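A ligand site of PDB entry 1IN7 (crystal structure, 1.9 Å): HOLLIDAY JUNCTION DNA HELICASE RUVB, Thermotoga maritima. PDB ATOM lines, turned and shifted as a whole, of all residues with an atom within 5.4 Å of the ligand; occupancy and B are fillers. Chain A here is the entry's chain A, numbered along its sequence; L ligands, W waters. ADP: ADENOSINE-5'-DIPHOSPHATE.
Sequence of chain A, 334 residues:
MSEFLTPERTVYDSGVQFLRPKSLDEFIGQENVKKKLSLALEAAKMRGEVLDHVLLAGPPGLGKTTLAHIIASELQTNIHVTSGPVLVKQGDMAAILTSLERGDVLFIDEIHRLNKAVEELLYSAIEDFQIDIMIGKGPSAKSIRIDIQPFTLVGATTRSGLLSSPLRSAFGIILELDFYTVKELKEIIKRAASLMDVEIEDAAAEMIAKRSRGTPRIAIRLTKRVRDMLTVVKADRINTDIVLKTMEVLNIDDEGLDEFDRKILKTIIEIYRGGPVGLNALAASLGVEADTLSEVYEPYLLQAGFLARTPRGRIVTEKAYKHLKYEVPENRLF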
ATOM      1  N   LEU A  19     -25.370  -3.636  23.893  1.00  0.00           N
ATOM      2  CA  LEU A  19     -24.280  -4.004  24.799  1.00  0.00           C
ATOM      3  C   LEU A  19     -22.967  -4.340  24.105  1.00  0.00           C
ATOM      4  O   LEU A  19     -22.049  -4.885  24.721  1.00  0.00           O
ATOM      5  CB  LEU A  19     -24.702  -5.194  25.666  1.00  0.00           C
ATOM      6  CG  LEU A  19     -25.993  -5.014  26.463  1.00  0.00           C
ATOM      7  CD1 LEU A  19     -26.409  -6.339  27.059  1.00  0.00           C
ATOM      8  CD2 LEU A  19     -25.792  -3.960  27.543  1.00  0.00           C
ATOM      9  N   ARG A  20     -22.873  -4.029  22.820  1.00  0.00           N
ATOM     10  CA  ARG A  20     -21.656  -4.327  22.065  1.00  0.00           C
ATOM     11  C   ARG A  20     -20.697  -3.150  21.952  1.00  0.00           C
ATOM     12  O   ARG A  20     -21.087  -2.052  21.534  1.00  0.00           O
ATOM     13  CB  ARG A  20     -22.034  -4.855  20.671  1.00  0.00           C
ATOM     14  CG  ARG A  20     -20.858  -5.147  19.766  1.00  0.00           C
ATOM     15  CD  ARG A  20     -21.278  -5.954  18.537  1.00  0.00           C
ATOM     16  NE  ARG A  20     -21.557  -7.346  18.875  1.00  0.00           N
ATOM     17  CZ  ARG A  20     -21.828  -8.301  17.997  1.00  0.00           C
ATOM     18  NH1 ARG A  20     -21.870  -8.020  16.698  1.00  0.00           N
ATOM     19  NH2 ARG A  20     -22.057  -9.548  18.410  1.00  0.00           N
ATOM     20  N   PRO A  21     -19.423  -3.346  22.356  1.00  0.00           N
ATOM     21  CA  PRO A  21     -18.378  -2.315  22.294  1.00  0.00           C
ATOM     22  C   PRO A  21     -18.255  -1.784  20.878  1.00  0.00           C
ATOM     23  O   PRO A  21     -18.180  -2.561  19.927  1.00  0.00           O
ATOM     24  CB  PRO A  21     -17.127  -3.062  22.722  1.00  0.00           C
ATOM     25  CG  PRO A  21     -17.644  -4.064  23.682  1.00  0.00           C
ATOM     26  CD  PRO A  21     -18.918  -4.565  23.018  1.00  0.00           C
ATOM     27  N   GLU A  26     -13.837   0.795  24.572  1.00  0.00           N
ATOM     28  CA  GLU A  26     -14.990   0.210  25.259  1.00  0.00           C
ATOM     29  C   GLU A  26     -14.876  -1.304  25.380  1.00  0.00           C
ATOM     30  O   GLU A  26     -15.737  -1.954  25.968  1.00  0.00           O
ATOM     31  CB  GLU A  26     -16.274   0.537  24.498  1.00  0.00           C
ATOM     32  CG  GLU A  26     -16.619   2.017  24.466  1.00  0.00           C
ATOM     33  CD  GLU A  26     -17.898   2.297  23.721  1.00  0.00           C
ATOM     34  OE1 GLU A  26     -18.271   3.485  23.623  1.00  0.00           O
ATOM     35  OE2 GLU A  26     -18.537   1.343  23.224  1.00  0.00           O
ATOM     36  N   PHE A  27     -13.800  -1.851  24.824  1.00  0.00           N
ATOM     37  CA  PHE A  27     -13.565  -3.296  24.835  1.00  0.00           C
ATOM     38  C   PHE A  27     -12.747  -3.670  26.070  1.00  0.00           C
ATOM     39  O   PHE A  27     -11.544  -3.443  26.116  1.00  0.00           O
ATOM     40  CB  PHE A  27     -12.826  -3.685  23.551  1.00  0.00           C
ATOM     41  CG  PHE A  27     -12.930  -5.143  23.197  1.00  0.00           C
ATOM     42  CD1 PHE A  27     -12.013  -6.064  23.680  1.00  0.00           C
ATOM     43  CD2 PHE A  27     -13.954  -5.588  22.354  1.00  0.00           C
ATOM     44  CE1 PHE A  27     -12.093  -7.422  23.308  1.00  0.00           C
ATOM     45  CE2 PHE A  27     -14.042  -6.930  21.985  1.00  0.00           C
ATOM     46  CZ  PHE A  27     -13.115  -7.845  22.460  1.00  0.00           C
ATOM     47  N   ILE A  28     -13.412  -4.243  27.072  1.00  0.00           N
ATOM     48  CA  ILE A  28     -12.734  -4.634  28.309  1.00  0.00           C
ATOM     49  C   ILE A  28     -11.886  -5.898  28.138  1.00  0.00           C
ATOM     50  O   ILE A  28     -12.277  -6.808  27.418  1.00  0.00           O
ATOM     51  CB  ILE A  28     -13.749  -4.850  29.445  1.00  0.00           C
ATOM     52  CG1 ILE A  28     -14.458  -3.530  29.763  1.00  0.00           C
ATOM     53  CG2 ILE A  28     -13.043  -5.391  30.683  1.00  0.00           C
ATOM     54  CD1 ILE A  28     -15.594  -3.653  30.741  1.00  0.00           C
ATOM     55  N   GLY A  29     -10.736  -5.942  28.807  1.00  0.00           N
ATOM     56  CA  GLY A  29      -9.869  -7.101  28.730  1.00  0.00           C
ATOM     57  C   GLY A  29      -9.135  -7.262  27.411  1.00  0.00           C
ATOM     58  O   GLY A  29      -9.142  -6.354  26.583  1.00  0.00           O
ATOM     59  N   PRO A  59     -12.324 -19.298  21.351  1.00  0.00           N
ATOM     60  CA  PRO A  59     -13.650 -19.836  21.646  1.00  0.00           C
ATOM     61  C   PRO A  59     -14.748 -18.815  21.355  1.00  0.00           C
ATOM     62  O   PRO A  59     -14.511 -17.608  21.294  1.00  0.00           O
ATOM     63  CB  PRO A  59     -13.563 -20.158  23.142  1.00  0.00           C
ATOM     64  CG  PRO A  59     -12.147 -20.570  23.300  1.00  0.00           C
ATOM     65  CD  PRO A  59     -11.401 -19.527  22.479  1.00  0.00           C
ATOM     66  N   PRO A  60     -15.967 -19.309  21.147  1.00  0.00           N
ATOM     67  CA  PRO A  60     -17.120 -18.452  20.853  1.00  0.00           C
ATOM     68  C   PRO A  60     -17.518 -17.544  22.019  1.00  0.00           C
ATOM     69  O   PRO A  60     -17.326 -17.896  23.194  1.00  0.00           O
ATOM     70  CB  PRO A  60     -18.220 -19.453  20.507  1.00  0.00           C
ATOM     71  CG  PRO A  60     -17.841 -20.658  21.333  1.00  0.00           C
ATOM     72  CD  PRO A  60     -16.349 -20.736  21.140  1.00  0.00           C
ATOM     73  N   GLY A  61     -18.031 -16.368  21.690  1.00  0.00           N
ATOM     74  CA  GLY A  61     -18.479 -15.416  22.690  1.00  0.00           C
ATOM     75  C   GLY A  61     -17.406 -14.551  23.329  1.00  0.00           C
ATOM     76  O   GLY A  61     -17.691 -13.833  24.295  1.00  0.00           O
ATOM     77  N   LEU A  62     -16.200 -14.578  22.779  1.00  0.00           N
ATOM     78  CA  LEU A  62     -15.079 -13.819  23.323  1.00  0.00           C
ATOM     79  C   LEU A  62     -14.842 -12.459  22.649  1.00  0.00           C
ATOM     80  O   LEU A  62     -13.884 -11.767  22.991  1.00  0.00           O
ATOM     81  CB  LEU A  62     -13.783 -14.649  23.241  1.00  0.00           C
ATOM     82  CG  LEU A  62     -13.758 -15.963  24.047  1.00  0.00           C
ATOM     83  CD1 LEU A  62     -12.365 -16.609  23.902  1.00  0.00           C
ATOM     84  CD2 LEU A  62     -14.047 -15.681  25.533  1.00  0.00           C
ATOM     85  N   GLY A  63     -15.705 -12.087  21.718  1.00  0.00           N
ATOM     86  CA  GLY A  63     -15.582 -10.790  21.050  1.00  0.00           C
ATOM     87  C   GLY A  63     -14.907 -10.684  19.692  1.00  0.00           C
ATOM     88  O   GLY A  63     -14.515  -9.580  19.277  1.00  0.00           O
ATOM     89  N   LYS A  64     -14.760 -11.809  18.996  1.00  0.00           N
ATOM     90  CA  LYS A  64     -14.134 -11.800  17.677  1.00  0.00           C
ATOM     91  C   LYS A  64     -14.986 -10.948  16.725  1.00  0.00           C
ATOM     92  O   LYS A  64     -14.487 -10.042  16.074  1.00  0.00           O
ATOM     93  CB  LYS A  64     -13.983 -13.250  17.159  1.00  0.00           C
ATOM     94  CG  LYS A  64     -13.015 -14.109  18.009  1.00  0.00           C
ATOM     95  CD  LYS A  64     -12.757 -15.514  17.441  1.00  0.00           C
ATOM     96  CE  LYS A  64     -14.039 -16.304  17.218  1.00  0.00           C
ATOM     97  NZ  LYS A  64     -14.754 -16.617  18.478  1.00  0.00           N
ATOM     98  N   THR A  65     -16.279 -11.254  16.656  1.00  0.00           N
ATOM     99  CA  THR A  65     -17.188 -10.493  15.818  1.00  0.00           C
ATOM    100  C   THR A  65     -17.149  -9.001  16.199  1.00  0.00           C
ATOM    101  O   THR A  65     -17.137  -8.126  15.333  1.00  0.00           O
ATOM    102  CB  THR A  65     -18.636 -11.005  15.963  1.00  0.00           C
ATOM    103  OG1 THR A  65     -18.726 -12.329  15.414  1.00  0.00           O
ATOM    104  CG2 THR A  65     -19.612 -10.082  15.253  1.00  0.00           C
ATOM    105  N   THR A  66     -17.131  -8.738  17.500  1.00  0.00           N
ATOM    106  CA  THR A  66     -17.082  -7.372  18.005  1.00  0.00           C
ATOM    107  C   THR A  66     -15.835  -6.628  17.515  1.00  0.00           C
ATOM    108  O   THR A  66     -15.919  -5.464  17.118  1.00  0.00           O
ATOM    109  CB  THR A  66     -17.128  -7.362  19.544  1.00  0.00           C
ATOM    110  OG1 THR A  66     -18.389  -7.908  19.991  1.00  0.00           O
ATOM    111  CG2 THR A  66     -16.988  -5.953  20.082  1.00  0.00           C
ATOM    112  N   LEU A  67     -14.695  -7.294  17.561  1.00  0.00           N
ATOM    113  CA  LEU A  67     -13.458  -6.691  17.096  1.00  0.00           C
ATOM    114  C   LEU A  67     -13.515  -6.430  15.587  1.00  0.00           C
ATOM    115  O   LEU A  67     -13.030  -5.398  15.112  1.00  0.00           O
ATOM    116  CB  LEU A  67     -12.256  -7.573  17.434  1.00  0.00           C
ATOM    117  CG  LEU A  67     -11.894  -7.611  18.929  1.00  0.00           C
ATOM    118  CD1 LEU A  67     -10.808  -8.649  19.184  1.00  0.00           C
ATOM    119  CD2 LEU A  67     -11.401  -6.230  19.365  1.00  0.00           C
ATOM    120  N   ASP A 109     -16.720 -15.144   9.189  1.00  0.00           N
ATOM    121  CA  ASP A 109     -16.778 -15.917  10.420  1.00  0.00           C
ATOM    122  C   ASP A 109     -16.710 -17.399  10.021  1.00  0.00           C
ATOM    123  O   ASP A 109     -17.103 -17.753   8.904  1.00  0.00           O
ATOM    124  CB  ASP A 109     -18.083 -15.596  11.146  1.00  0.00           C
ATOM    125  CG  ASP A 109     -18.147 -16.203  12.534  1.00  0.00           C
ATOM    126  OD1 ASP A 109     -17.114 -16.195  13.243  1.00  0.00           O
ATOM    127  OD2 ASP A 109     -19.233 -16.684  12.923  1.00  0.00           O
ATOM    128  N   TYR A 180     -11.420 -14.662  29.459  1.00  0.00           N
ATOM    129  CA  TYR A 180     -11.211 -13.463  30.245  1.00  0.00           C
ATOM    130  C   TYR A 180     -11.064 -13.828  31.715  1.00  0.00           C
ATOM    131  O   TYR A 180     -11.492 -14.902  32.150  1.00  0.00           O
ATOM    132  CB  TYR A 180     -12.402 -12.512  30.101  1.00  0.00           C
ATOM    133  CG  TYR A 180     -12.564 -11.900  28.725  1.00  0.00           C
ATOM    134  CD1 TYR A 180     -12.850 -12.694  27.619  1.00  0.00           C
ATOM    135  CD2 TYR A 180     -12.442 -10.533  28.547  1.00  0.00           C
ATOM    136  CE1 TYR A 180     -13.014 -12.111  26.343  1.00  0.00           C
ATOM    137  CE2 TYR A 180     -12.602  -9.940  27.293  1.00  0.00           C
ATOM    138  CZ  TYR A 180     -12.885 -10.736  26.200  1.00  0.00           C
ATOM    139  OH  TYR A 180     -13.025 -10.108  24.981  1.00  0.00           O
ATOM    140  N   ILE A 188     -17.312  -6.298  32.849  1.00  0.00           N
ATOM    141  CA  ILE A 188     -18.253  -6.376  31.732  1.00  0.00           C
ATOM    142  C   ILE A 188     -19.686  -6.501  32.269  1.00  0.00           C
ATOM    143  O   ILE A 188     -20.634  -5.938  31.714  1.00  0.00           O
ATOM    144  CB  ILE A 188     -17.898  -7.571  30.803  1.00  0.00           C
ATOM    145  CG1 ILE A 188     -16.599  -7.268  30.052  1.00  0.00           C
ATOM    146  CG2 ILE A 188     -19.027  -7.851  29.812  1.00  0.00           C
ATOM    147  CD1 ILE A 188     -15.933  -8.482  29.426  1.00  0.00           C
ATOM    148  N   ARG A 191     -20.965  -3.180  33.692  1.00  0.00           N
ATOM    149  CA  ARG A 191     -21.234  -2.346  32.532  1.00  0.00           C
ATOM    150  C   ARG A 191     -22.566  -2.715  31.881  1.00  0.00           C
ATOM    151  O   ARG A 191     -23.331  -1.826  31.497  1.00  0.00           O
ATOM    152  CB  ARG A 191     -20.085  -2.492  31.524  1.00  0.00           C
ATOM    153  CG  ARG A 191     -20.317  -1.795  30.203  1.00  0.00           C
ATOM    154  CD  ARG A 191     -19.054  -1.882  29.363  1.00  0.00           C
ATOM    155  NE  ARG A 191     -19.197  -1.243  28.058  1.00  0.00           N
ATOM    156  CZ  ARG A 191     -19.832  -1.785  27.024  1.00  0.00           C
ATOM    157  NH1 ARG A 191     -19.908  -1.121  25.874  1.00  0.00           N
ATOM    158  NH2 ARG A 191     -20.374  -2.989  27.115  1.00  0.00           N
ATOM    159  N   PRO A 216     -17.525 -13.416  27.900  1.00  0.00           N
ATOM    160  CA  PRO A 216     -18.368 -12.225  27.966  1.00  0.00           C
ATOM    161  C   PRO A 216     -19.824 -12.521  27.579  1.00  0.00           C
ATOM    162  O   PRO A 216     -20.728 -12.106  28.284  1.00  0.00           O
ATOM    163  CB  PRO A 216     -17.706 -11.278  26.980  1.00  0.00           C
ATOM    164  CG  PRO A 216     -16.252 -11.608  27.145  1.00  0.00           C
ATOM    165  CD  PRO A 216     -16.262 -13.127  27.193  1.00  0.00           C
ATOM    166  N   ARG A 217     -20.032 -13.232  26.476  1.00  0.00           N
ATOM    167  CA  ARG A 217     -21.381 -13.563  26.038  1.00  0.00           C
ATOM    168  C   ARG A 217     -22.173 -14.247  27.147  1.00  0.00           C
ATOM    169  O   ARG A 217     -23.333 -13.913  27.409  1.00  0.00           O
ATOM    170  CB  ARG A 217     -21.343 -14.453  24.800  1.00  0.00           C
ATOM    171  CG  ARG A 217     -22.706 -14.902  24.331  1.00  0.00           C
ATOM    172  CD  ARG A 217     -22.548 -15.853  23.160  1.00  0.00           C
ATOM    173  NE  ARG A 217     -22.211 -15.159  21.921  1.00  0.00           N
ATOM    174  CZ  ARG A 217     -21.771 -15.770  20.840  1.00  0.00           C
ATOM    175  NH1 ARG A 217     -21.590 -17.085  20.855  1.00  0.00           N
ATOM    176  NH2 ARG A 217     -21.519 -15.073  19.730  1.00  0.00           N
ATOM    177  N   ILE A 220     -22.910 -11.767  30.160  1.00  0.00           N
ATOM    178  CA  ILE A 220     -23.979 -10.830  29.839  1.00  0.00           C
ATOM    179  C   ILE A 220     -25.354 -11.507  29.884  1.00  0.00           C
ATOM    180  O   ILE A 220     -26.305 -10.936  30.426  1.00  0.00           O
ATOM    181  CB  ILE A 220     -23.745 -10.199  28.450  1.00  0.00           C
ATOM    182  CG1 ILE A 220     -22.458  -9.372  28.478  1.00  0.00           C
ATOM    183  CG2 ILE A 220     -24.908  -9.304  28.082  1.00  0.00           C
ATOM    184  CD1 ILE A 220     -21.984  -8.946  27.098  1.00  0.00           C
HETATM  185  PB  ADP L   1     -17.568 -14.151  19.045  1.00  0.00           P
HETATM  186  O1B ADP L   1     -16.222 -14.427  19.533  1.00  0.00           O
HETATM  187  O2B ADP L   1     -17.601 -13.562  17.614  1.00  0.00           O
HETATM  188  O3B ADP L   1     -18.509 -15.383  19.127  1.00  0.00           O
HETATM  189  PA  ADP L   1     -18.987 -11.710  19.901  1.00  0.00           P
HETATM  190  O1A ADP L   1     -18.078 -10.654  19.357  1.00  0.00           O
HETATM  191  O2A ADP L   1     -20.172 -11.912  19.056  1.00  0.00           O
HETATM  192  O3A ADP L   1     -18.247 -13.180  20.015  1.00  0.00           O
HETATM  193  O5' ADP L   1     -19.442 -11.419  21.371  1.00  0.00           O
HETATM  194  C5' ADP L   1     -20.458 -11.743  22.248  1.00  0.00           C
HETATM  195  C4' ADP L   1     -21.156 -10.815  22.977  1.00  0.00           C
HETATM  196  O4' ADP L   1     -20.299 -10.525  24.012  1.00  0.00           O
HETATM  197  C3' ADP L   1     -21.283  -9.408  22.359  1.00  0.00           C
HETATM  198  O3' ADP L   1     -22.557  -9.155  22.831  1.00  0.00           O
HETATM  199  C2' ADP L   1     -20.487  -8.431  23.010  1.00  0.00           C
HETATM  200  O2' ADP L   1     -21.102  -7.129  22.836  1.00  0.00           O
HETATM  201  C1' ADP L   1     -19.843  -9.302  24.186  1.00  0.00           C
HETATM  202  N9  ADP L   1     -18.503  -9.088  24.329  1.00  0.00           N
HETATM  203  C8  ADP L   1     -17.443  -9.761  23.802  1.00  0.00           C
HETATM  204  N7  ADP L   1     -16.319  -9.314  24.138  1.00  0.00           N
HETATM  205  C5  ADP L   1     -16.622  -8.262  24.974  1.00  0.00           C
HETATM  206  C6  ADP L   1     -15.795  -7.321  25.709  1.00  0.00           C
HETATM  207  N6  ADP L   1     -14.446  -7.411  25.645  1.00  0.00           N
HETATM  208  N1  ADP L   1     -16.422  -6.315  26.509  1.00  0.00           N
HETATM  209  C2  ADP L   1     -17.805  -6.241  26.572  1.00  0.00           C
HETATM  210  N3  ADP L   1     -18.654  -7.101  25.895  1.00  0.00           N
HETATM  211  C4  ADP L   1     -18.007  -8.095  25.113  1.00  0.00           C
HETATM  212  O   HOH W   1     -17.007 -15.505  15.785  1.00  0.00           O
HETATM  213  O   HOH W   2     -21.417 -13.928  17.241  1.00  0.00           O
HETATM  214  O   HOH W   3     -21.028  -6.077  26.833  1.00  0.00           O
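CD of Pro 21 touches O2' of the ligand (3.4 Å). Phe 27 touches the ligand. C of Pro 60 touches O3B of the ligand (3.7 Å). Ile 188 touches the ligand (CD1 to N1, 3.7 Å). Pro 216 touches the ligand (CB to N9, 3.5 Å). CD1 of Ile 220 touches C1' of the ligand (3.6 Å). Hydrophobic or aromatic side chains within 4 Å of the ligand: Pro 21, Phe 27, Tyr 180, Ile 188, Pro 216 and Ile 220. Within 4 Å of the ligand: Leu 19, Arg 20, Pro 21, Phe 27, Ile 28, Pro 60, Gly 61, Leu 62, Gly 63, Lys 64, Thr 65, Thr 66, Tyr 180, Ile 188, Pro 216, Arg 217 and Ile 220.
The guanidinium group (NH2) of Arg 20 lies within salt-bridge range of an oxygen (O2A) of the ligand, 3.1 Å away. The backbone NH (N) of Thr 66 sits at hydrogen-bond distance from an oxygen (O1A) of the ligand (2.8 Å). An oxygen (O3B) of the ligand is in hydrogen-bond range of the backbone NH of Gly 61, 2.8 Å away. NZ of Lys 64 is in salt-bridge range of O1B of the ligand (2.8 Å). The backbone NH (N) of Thr 65 lies within hydrogen-bond range of an oxygen (O2B) of the ligand (2.8 Å). The backbone carbonyl oxygen (O) of Ile 28 lies within hydrogen-bond range of a nitrogen (N6) of the ligand (2.9 Å). The side-chain hydroxyl (OG1) of Thr 66 is in hydrogen-bond range of an oxygen (O1A) of the ligand, at 2.8 Å. The side-chain hydroxyl (OG1) of Thr 65 lies within hydrogen-bond range of an oxygen (O2B) of the ligand, 2.8 Å away. O1B of the ligand sits at hydrogen-bond distance from N of Gly 63. An oxygen (O3B) of the ligand is in salt-bridge range of the guanidinium group of Arg 217. The side-chain hydroxyl of Tyr 180 sits at hydrogen-bond distance from a nitrogen (N6) of the ligand, 3.1 Å away. The backbone NH (N) of Lys 64 is in hydrogen-bond range of an oxygen (O1B) of the ligand (3.0 Å). The backbone carbonyl oxygen of Leu 19 sits at hydrogen-bond distance from an oxygen (O2') of the ligand. The backbone NH (N) of Leu 62 sits at hydrogen-bond distance from an oxygen (O1B) of the ligand (3.2 Å).
The backbone carbonyl oxygen (O) of Leu 19 lies within hydrogen-bond range of the guanidinium group (NH2) of Arg 191 (3.5 Å). The side-chain amino group of Lys 64 is in hydrogen-bond range of the backbone carbonyl oxygen of Pro 59 (3.0 Å). The guanidinium group (NE) of Arg 20 is in hydrogen-bond range of the side-chain hydroxyl (OG1) of Thr 66, 3.4 Å away. The backbone carbonyl oxygen of Gly 61 lies within hydrogen-bond range of the backbone NH of Arg 217, 3.3 Å away. The side-chain hydroxyl (OH) of Tyr 180 is in hydrogen-bond range of the backbone carbonyl oxygen (O) of Leu 62, at 2.7 Å.
Water W1 lies within hydrogen-bond range of the side-chain carboxylate (OD1) of Asp 109 and an oxygen (O2B) of the ligand. Water W3 lies within hydrogen-bond range of O of Leu 19 (2.6 Å), N3 of the ligand (2.8 Å) and NH2 of Arg 191 (3.2 Å). Water W2 bridges the guanidinium group (NH2) of Arg 217 (2.7 Å) and an oxygen (O2A) of the ligand (3.0 Å).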
